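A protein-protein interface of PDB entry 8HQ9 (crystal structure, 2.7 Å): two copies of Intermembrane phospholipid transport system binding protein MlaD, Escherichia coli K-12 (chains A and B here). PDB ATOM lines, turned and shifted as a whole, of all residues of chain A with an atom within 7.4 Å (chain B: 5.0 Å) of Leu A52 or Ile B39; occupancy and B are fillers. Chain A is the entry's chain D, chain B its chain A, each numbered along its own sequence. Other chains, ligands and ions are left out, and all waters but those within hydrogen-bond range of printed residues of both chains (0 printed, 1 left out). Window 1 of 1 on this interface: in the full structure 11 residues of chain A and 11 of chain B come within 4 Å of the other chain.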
ATOM      1  N   PHE A  25     -10.786  13.192   6.477  1.00  0.00           N
ATOM      2  CA  PHE A  25     -11.334  13.429   7.831  1.00  0.00           C
ATOM      3  C   PHE A  25     -10.580  14.580   8.502  1.00  0.00           C
ATOM      4  O   PHE A  25      -9.432  14.852   8.133  1.00  0.00           O
ATOM      5  CB  PHE A  25     -11.247  12.147   8.644  1.00  0.00           C
ATOM      6  CG  PHE A  25     -12.056  10.998   8.097  1.00  0.00           C
ATOM      7  CD1 PHE A  25     -11.556  10.225   7.053  1.00  0.00           C
ATOM      8  CD2 PHE A  25     -13.281  10.656   8.643  1.00  0.00           C
ATOM      9  CE1 PHE A  25     -12.278   9.150   6.559  1.00  0.00           C
ATOM     10  CE2 PHE A  25     -13.986   9.569   8.168  1.00  0.00           C
ATOM     11  CZ  PHE A  25     -13.509   8.844   7.109  1.00  0.00           C
ATOM     12  N   ASP A  26     -11.210  15.249   9.460  1.00  0.00           N
ATOM     13  CA  ASP A  26     -10.489  16.166  10.371  1.00  0.00           C
ATOM     14  C   ASP A  26      -9.618  15.322  11.298  1.00  0.00           C
ATOM     15  O   ASP A  26      -8.494  15.713  11.559  1.00  0.00           O
ATOM     16  CB  ASP A  26     -11.468  17.061  11.118  1.00  0.00           C
ATOM     17  CG  ASP A  26     -12.177  18.034  10.199  1.00  0.00           C
ATOM     18  OD1 ASP A  26     -11.509  18.725   9.378  1.00  0.00           O
ATOM     19  OD2 ASP A  26     -13.395  18.084  10.316  1.00  0.00           O
ATOM     20  N   ASN A  27     -10.116  14.176  11.747  1.00  0.00           N
ATOM     21  CA  ASN A  27      -9.417  13.337  12.739  1.00  0.00           C
ATOM     22  C   ASN A  27      -9.759  11.870  12.513  1.00  0.00           C
ATOM     23  O   ASN A  27     -10.919  11.554  12.576  1.00  0.00           O
ATOM     24  CB  ASN A  27      -9.773  13.774  14.161  1.00  0.00           C
ATOM     25  CG  ASN A  27      -8.792  13.193  15.153  1.00  0.00           C
ATOM     26  OD1 ASN A  27      -8.858  12.019  15.492  1.00  0.00           O
ATOM     27  ND2 ASN A  27      -7.788  13.960  15.518  1.00  0.00           N
ATOM     28  N   ILE A  28      -8.757  11.019  12.313  1.00  0.00           N
ATOM     29  CA  ILE A  28      -8.970   9.563  12.035  1.00  0.00           C
ATOM     30  C   ILE A  28      -8.784   8.741  13.318  1.00  0.00           C
ATOM     31  O   ILE A  28      -8.853   7.493  13.224  1.00  0.00           O
ATOM     32  CB  ILE A  28      -8.091   9.052  10.882  1.00  0.00           C
ATOM     33  CG1 ILE A  28      -6.599   9.249  11.111  1.00  0.00           C
ATOM     34  CG2 ILE A  28      -8.513   9.716   9.606  1.00  0.00           C
ATOM     35  CD1 ILE A  28      -5.883   8.071  11.684  1.00  0.00           C
ATOM     36  N   ASP A  49      -4.472   2.898   2.627  1.00  0.00           N
ATOM     37  CA  ASP A  49      -3.443   3.891   2.994  1.00  0.00           C
ATOM     38  C   ASP A  49      -4.067   5.011   3.826  1.00  0.00           C
ATOM     39  O   ASP A  49      -5.238   5.265   3.670  1.00  0.00           O
ATOM     40  CB  ASP A  49      -2.750   4.448   1.754  1.00  0.00           C
ATOM     41  CG  ASP A  49      -1.598   5.382   2.126  1.00  0.00           C
ATOM     42  OD1 ASP A  49      -0.590   4.903   2.666  1.00  0.00           O
ATOM     43  OD2 ASP A  49      -1.743   6.595   1.920  1.00  0.00           O
ATOM     44  N   ILE A  50      -3.259   5.591   4.699  1.00  0.00           N
ATOM     45  CA  ILE A  50      -3.532   6.860   5.423  1.00  0.00           C
ATOM     46  C   ILE A  50      -2.308   7.754   5.225  1.00  0.00           C
ATOM     47  O   ILE A  50      -1.185   7.291   5.501  1.00  0.00           O
ATOM     48  CB  ILE A  50      -3.809   6.637   6.903  1.00  0.00           C
ATOM     49  CG1 ILE A  50      -4.933   5.626   7.120  1.00  0.00           C
ATOM     50  CG2 ILE A  50      -4.117   7.974   7.532  1.00  0.00           C
ATOM     51  CD1 ILE A  50      -5.378   5.430   8.586  1.00  0.00           C
ATOM     52  N   THR A  51      -2.501   8.950   4.694  1.00  0.00           N
ATOM     53  CA  THR A  51      -1.433   9.948   4.748  1.00  0.00           C
ATOM     54  C   THR A  51      -2.045  11.232   5.252  1.00  0.00           C
ATOM     55  O   THR A  51      -3.242  11.465   4.998  1.00  0.00           O
ATOM     56  CB  THR A  51      -0.702  10.178   3.425  1.00  0.00           C
ATOM     57  OG1 THR A  51      -1.551  11.058   2.684  1.00  0.00           O
ATOM     58  CG2 THR A  51      -0.366   8.880   2.723  1.00  0.00           C
ATOM     59  N   LEU A  52      -1.187  12.002   5.906  1.00  0.00           N
ATOM     60  CA  LEU A  52      -1.504  13.366   6.291  1.00  0.00           C
ATOM     61  C   LEU A  52      -1.004  14.245   5.159  1.00  0.00           C
ATOM     62  O   LEU A  52       0.187  14.133   4.826  1.00  0.00           O
ATOM     63  CB  LEU A  52      -0.783  13.633   7.601  1.00  0.00           C
ATOM     64  CG  LEU A  52      -1.126  14.976   8.219  1.00  0.00           C
ATOM     65  CD1 LEU A  52      -2.579  14.976   8.682  1.00  0.00           C
ATOM     66  CD2 LEU A  52      -0.151  15.263   9.340  1.00  0.00           C
ATOM     67  N   ASP A  53      -1.901  15.035   4.566  1.00  0.00           N
ATOM     68  CA  ASP A  53      -1.555  15.984   3.493  1.00  0.00           C
ATOM     69  C   ASP A  53      -0.675  17.073   4.094  1.00  0.00           C
ATOM     70  O   ASP A  53      -1.136  17.831   4.954  1.00  0.00           O
ATOM     71  CB  ASP A  53      -2.815  16.589   2.887  1.00  0.00           C
ATOM     72  CG  ASP A  53      -2.546  17.488   1.690  1.00  0.00           C
ATOM     73  OD1 ASP A  53      -1.551  18.291   1.685  1.00  0.00           O
ATOM     74  OD2 ASP A  53      -3.367  17.374   0.745  1.00  0.00           O
ATOM     75  N   PRO A  54       0.587  17.238   3.642  1.00  0.00           N
ATOM     76  CA  PRO A  54       1.446  18.258   4.247  1.00  0.00           C
ATOM     77  C   PRO A  54       0.893  19.674   4.019  1.00  0.00           C
ATOM     78  O   PRO A  54       1.202  20.561   4.793  1.00  0.00           O
ATOM     79  CB  PRO A  54       2.813  18.038   3.607  1.00  0.00           C
ATOM     80  CG  PRO A  54       2.705  16.696   2.859  1.00  0.00           C
ATOM     81  CD  PRO A  54       1.233  16.471   2.563  1.00  0.00           C
ATOM     82  N   LYS A  55       0.039  19.858   3.009  1.00  0.00           N
ATOM     83  CA  LYS A  55      -0.470  21.199   2.631  1.00  0.00           C
ATOM     84  C   LYS A  55      -1.701  21.579   3.473  1.00  0.00           C
ATOM     85  O   LYS A  55      -1.788  22.720   3.877  1.00  0.00           O
ATOM     86  CB  LYS A  55      -0.684  21.245   1.112  1.00  0.00           C
ATOM     87  CG  LYS A  55       0.563  20.906   0.277  1.00  0.00           C
ATOM     88  CD  LYS A  55       0.836  21.755  -0.974  1.00  0.00           C
ATOM     89  CE  LYS A  55      -0.048  21.340  -2.140  1.00  0.00           C
ATOM     90  NZ  LYS A  55       0.480  21.843  -3.420  1.00  0.00           N
ATOM     91  N   THR A  56      -2.623  20.661   3.748  1.00  0.00           N
ATOM     92  CA  THR A  56      -3.898  20.954   4.469  1.00  0.00           C
ATOM     93  C   THR A  56      -3.857  20.468   5.926  1.00  0.00           C
ATOM     94  O   THR A  56      -4.709  20.901   6.718  1.00  0.00           O
ATOM     95  CB  THR A  56      -5.077  20.331   3.708  1.00  0.00           C
ATOM     96  OG1 THR A  56      -4.982  18.901   3.727  1.00  0.00           O
ATOM     97  CG2 THR A  56      -5.136  20.824   2.270  1.00  0.00           C
ATOM     98  N   TYR A  57      -2.910  19.581   6.251  1.00  0.00           N
ATOM     99  CA  TYR A  57      -2.773  18.850   7.540  1.00  0.00           C
ATOM    100  C   TYR A  57      -4.084  18.112   7.821  1.00  0.00           C
ATOM    101  O   TYR A  57      -4.414  17.894   8.985  1.00  0.00           O
ATOM    102  CB  TYR A  57      -2.308  19.789   8.659  1.00  0.00           C
ATOM    103  CG  TYR A  57      -0.858  20.217   8.575  1.00  0.00           C
ATOM    104  CD1 TYR A  57       0.176  19.301   8.617  1.00  0.00           C
ATOM    105  CD2 TYR A  57      -0.516  21.534   8.370  1.00  0.00           C
ATOM    106  CE1 TYR A  57       1.501  19.673   8.487  1.00  0.00           C
ATOM    107  CE2 TYR A  57       0.802  21.936   8.256  1.00  0.00           C
ATOM    108  CZ  TYR A  57       1.821  21.004   8.337  1.00  0.00           C
ATOM    109  OH  TYR A  57       3.131  21.386   8.219  1.00  0.00           O
ATOM    110  N   LEU A  58      -4.794  17.689   6.778  1.00  0.00           N
ATOM    111  CA  LEU A  58      -5.947  16.786   6.936  1.00  0.00           C
ATOM    112  C   LEU A  58      -5.544  15.379   6.521  1.00  0.00           C
ATOM    113  O   LEU A  58      -4.887  15.179   5.497  1.00  0.00           O
ATOM    114  CB  LEU A  58      -7.120  17.280   6.101  1.00  0.00           C
ATOM    115  CG  LEU A  58      -7.608  18.676   6.443  1.00  0.00           C
ATOM    116  CD1 LEU A  58      -8.796  19.008   5.548  1.00  0.00           C
ATOM    117  CD2 LEU A  58      -8.024  18.740   7.910  1.00  0.00           C
ATOM    118  N   PRO A  59      -5.876  14.367   7.356  1.00  0.00           N
ATOM    119  CA  PRO A  59      -5.680  12.971   6.973  1.00  0.00           C
ATOM    120  C   PRO A  59      -6.580  12.569   5.800  1.00  0.00           C
ATOM    121  O   PRO A  59      -7.752  12.926   5.764  1.00  0.00           O
ATOM    122  CB  PRO A  59      -6.059  12.176   8.222  1.00  0.00           C
ATOM    123  CG  PRO A  59      -6.890  13.146   9.048  1.00  0.00           C
ATOM    124  CD  PRO A  59      -6.345  14.519   8.741  1.00  0.00           C
ATOM    125  N   ARG A  60      -5.988  11.832   4.868  1.00  0.00           N
ATOM    126  CA  ARG A  60      -6.673  11.329   3.658  1.00  0.00           C
ATOM    127  C   ARG A  60      -6.555   9.821   3.713  1.00  0.00           C
ATOM    128  O   ARG A  60      -5.444   9.308   3.886  1.00  0.00           O
ATOM    129  CB  ARG A  60      -6.131  11.898   2.343  1.00  0.00           C
ATOM    130  CG  ARG A  60      -6.994  11.503   1.154  1.00  0.00           C
ATOM    131  CD  ARG A  60      -6.842  12.445  -0.015  1.00  0.00           C
ATOM    132  NE  ARG A  60      -5.974  11.834  -0.993  1.00  0.00           N
ATOM    133  CZ  ARG A  60      -6.350  11.440  -2.222  1.00  0.00           C
ATOM    134  NH1 ARG A  60      -7.602  11.614  -2.638  1.00  0.00           N
ATOM    135  NH2 ARG A  60      -5.449  10.880  -3.029  1.00  0.00           N
ATOM    136  N   VAL B  37       2.918  12.322  19.304  1.00  0.00           N
ATOM    137  CA  VAL B  37       2.299  13.615  18.922  1.00  0.00           C
ATOM    138  C   VAL B  37       1.584  13.392  17.593  1.00  0.00           C
ATOM    139  O   VAL B  37       2.254  12.904  16.651  1.00  0.00           O
ATOM    140  CB  VAL B  37       3.365  14.706  18.760  1.00  0.00           C
ATOM    141  CG1 VAL B  37       2.738  16.044  18.358  1.00  0.00           C
ATOM    142  CG2 VAL B  37       4.154  14.861  20.036  1.00  0.00           C
ATOM    143  N   SER B  38       0.291  13.715  17.515  1.00  0.00           N
ATOM    144  CA  SER B  38      -0.536  13.429  16.321  1.00  0.00           C
ATOM    145  C   SER B  38      -1.224  14.704  15.817  1.00  0.00           C
ATOM    146  O   SER B  38      -1.431  15.621  16.622  1.00  0.00           O
ATOM    147  CB  SER B  38      -1.510  12.340  16.598  1.00  0.00           C
ATOM    148  OG  SER B  38      -2.549  12.789  17.475  1.00  0.00           O
ATOM    149  N   ILE B  39      -1.500  14.739  14.513  1.00  0.00           N
ATOM    150  CA  ILE B  39      -2.359  15.732  13.840  1.00  0.00           C
ATOM    151  C   ILE B  39      -3.453  14.931  13.153  1.00  0.00           C
ATOM    152  O   ILE B  39      -3.129  14.006  12.403  1.00  0.00           O
ATOM    153  CB  ILE B  39      -1.550  16.577  12.850  1.00  0.00           C
ATOM    154  CG1 ILE B  39      -0.407  17.314  13.555  1.00  0.00           C
ATOM    155  CG2 ILE B  39      -2.448  17.551  12.104  1.00  0.00           C
ATOM    156  CD1 ILE B  39       0.451  18.178  12.615  1.00  0.00           C
ATOM    157  N   GLY B  40      -4.707  15.256  13.442  1.00  0.00           N
ATOM    158  CA  GLY B  40      -5.871  14.458  13.027  1.00  0.00           C
ATOM    159  C   GLY B  40      -5.665  12.966  13.252  1.00  0.00           C
ATOM    160  O   GLY B  40      -6.116  12.163  12.404  1.00  0.00           O
ATOM    161  N   GLY B  41      -5.017  12.580  14.345  1.00  0.00           N
ATOM    162  CA  GLY B  41      -4.803  11.165  14.683  1.00  0.00           C
ATOM    163  C   GLY B  41      -3.655  10.520  13.927  1.00  0.00           C
ATOM    164  O   GLY B  41      -3.471   9.299  14.081  1.00  0.00           O
ATOM    165  N   VAL B  42      -2.912  11.252  13.107  1.00  0.00           N
ATOM    166  CA  VAL B  42      -1.720  10.680  12.423  1.00  0.00           C
ATOM    167  C   VAL B  42      -0.500  11.129  13.202  1.00  0.00           C
ATOM    168  O   VAL B  42      -0.397  12.330  13.541  1.00  0.00           O
ATOM    169  CB  VAL B  42      -1.624  11.088  10.950  1.00  0.00           C
ATOM    170  CG1 VAL B  42      -0.415  10.446  10.313  1.00  0.00           C
ATOM    171  CG2 VAL B  42      -2.895  10.724  10.207  1.00  0.00           C
ATOM    172  N   VAL B  44       2.939  12.498  13.866  1.00  0.00           N
ATOM    173  CA  VAL B  44       3.913  13.450  13.259  1.00  0.00           C
ATOM    174  C   VAL B  44       5.149  13.613  14.159  1.00  0.00           C
ATOM    175  O   VAL B  44       6.078  14.282  13.709  1.00  0.00           O
ATOM    176  CB  VAL B  44       3.263  14.815  13.005  1.00  0.00           C
ATOM    177  CG1 VAL B  44       2.144  14.689  11.995  1.00  0.00           C
ATOM    178  CG2 VAL B  44       2.792  15.454  14.312  1.00  0.00           C
ATOM    179  N   TYR B  69       6.557  17.880   8.258  1.00  0.00           N
ATOM    180  CA  TYR B  69       5.394  18.643   8.774  1.00  0.00           C
ATOM    181  C   TYR B  69       5.904  19.979   9.333  1.00  0.00           C
ATOM    182  O   TYR B  69       6.094  20.098  10.546  1.00  0.00           O
ATOM    183  CB  TYR B  69       4.636  17.791   9.784  1.00  0.00           C
ATOM    184  CG  TYR B  69       4.288  16.413   9.275  1.00  0.00           C
ATOM    185  CD1 TYR B  69       3.451  16.246   8.178  1.00  0.00           C
ATOM    186  CD2 TYR B  69       4.818  15.274   9.869  1.00  0.00           C
ATOM    187  CE1 TYR B  69       3.130  14.984   7.707  1.00  0.00           C
ATOM    188  CE2 TYR B  69       4.518  14.003   9.394  1.00  0.00           C
ATOM    189  CZ  TYR B  69       3.656  13.857   8.317  1.00  0.00           C
ATOM    190  OH  TYR B  69       3.335  12.619   7.828  1.00  0.00           O
ATOM    191  N   ILE B  72       3.483  24.559  10.201  1.00  0.00           N
ATOM    192  CA  ILE B  72       2.476  24.564  11.293  1.00  0.00           C
ATOM    193  C   ILE B  72       2.425  25.963  11.895  1.00  0.00           C
ATOM    194  O   ILE B  72       3.434  26.441  12.401  1.00  0.00           O
ATOM    195  CB  ILE B  72       2.802  23.507  12.356  1.00  0.00           C
ATOM    196  CG1 ILE B  72       2.891  22.119  11.730  1.00  0.00           C
ATOM    197  CG2 ILE B  72       1.801  23.576  13.506  1.00  0.00           C
ATOM    198  CD1 ILE B  72       3.276  21.054  12.726  1.00  0.00           C
ATOM    199  N   LEU B  93      -1.828  17.776  18.347  1.00  0.00           N
ATOM    200  CA  LEU B  93      -1.498  19.102  17.789  1.00  0.00           C
ATOM    201  C   LEU B  93      -2.699  19.532  16.953  1.00  0.00           C
ATOM    202  O   LEU B  93      -3.021  18.825  15.961  1.00  0.00           O
ATOM    203  CB  LEU B  93      -0.213  18.991  16.966  1.00  0.00           C
ATOM    204  CG  LEU B  93       0.610  20.271  16.907  1.00  0.00           C
ATOM    205  CD1 LEU B  93       2.022  19.991  16.419  1.00  0.00           C
ATOM    206  CD2 LEU B  93      -0.060  21.286  15.998  1.00  0.00           C
ATOM    207  N   VAL B  95      -3.931  22.194  14.494  1.00  0.00           N
ATOM    208  CA  VAL B  95      -3.337  23.168  13.548  1.00  0.00           C
ATOM    209  C   VAL B  95      -4.192  24.438  13.514  1.00  0.00           C
ATOM    210  O   VAL B  95      -5.360  24.344  13.170  1.00  0.00           O
ATOM    211  CB  VAL B  95      -3.193  22.526  12.168  1.00  0.00           C
ATOM    212  CG1 VAL B  95      -2.702  23.536  11.158  1.00  0.00           C
ATOM    213  CG2 VAL B  95      -2.286  21.297  12.228  1.00  0.00           C
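N of Ile A28 lies within hydrogen-bond range of O of Gly B40, at 2.9 Å.
The side-chain amide nitrogen of Asn A27 lies close to the backbone NH of Gly B41 (3.3 Å).
N of Val B44 lies within hydrogen-bond range of O of Val B37 (2.9 Å).
The backbone NH of Phe A25 sits at hydrogen-bond distance from the backbone carbonyl oxygen of Pro A59, 3.1 Å away.
Among the printed residues, pairs that only touch across the chains: Asp A26 with Gly B40 (3.3 Å), Asn A27 with Gly B40 (3.2 Å), Ile A28 with Gly B41 (3.6 Å), Leu A52 with Ile B39 (3.9 Å), Leu A52 with Val B44 (3.6 Å), Leu A52 with Tyr B69 (3.7 Å), Tyr A57 with Ile B39 (3.7 Å), Tyr A57 with Tyr B69 (3.3 Å), Tyr A57 with Ile B72 (3.6 Å), Tyr A57 with Val B95 (3.9 Å) and Pro A59 with Gly B40 (3.6 Å).
Printed residues of chain B within 4 Å of Asp A26: Gly B40 (3.3 Å).
Leu A52 touches just these residues of chain B: Ile B39, Val B44 and Tyr B69.
Leu A58 touches none of the printed residues of chain B.
Printed residues of chain B within 4 Å of Pro A59: Gly B40.
Of chain A, only Leu A52 (3.9 Å) and Tyr A57 (3.7 Å) come within 4 Å of Ile B39.
Val B42 touches none of the printed residues of chain A.
Of the printed residues of chain A, Val B44 touches Leu A52 (3.6 Å).
Of the printed residues of chain A, Ile B72 touches Tyr A57 (3.6 Å).
Of the printed residues of chain A, Val B95 touches Tyr A57.
The nearest printed residue of chain A that does not touch Val B44 is Tyr A57 (6.0 Å).
Of the 11 printed residues of chain B, 7 touch a printed residue of chain A.
Of the 16 printed residues of chain A, 6 touch a printed residue of chain B.
Hydrophobic or aromatic side chains of chain A that line the printed part of chain B: Ile A28, Leu A52, Tyr A57 and Pro A59.
Among the printed residues, 13 pairs touch across the chains.
No position is printed for both chains.
Of the 13 pairs that touch across the chains among the printed residues, none has its exchanged pair printed and touching as well.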
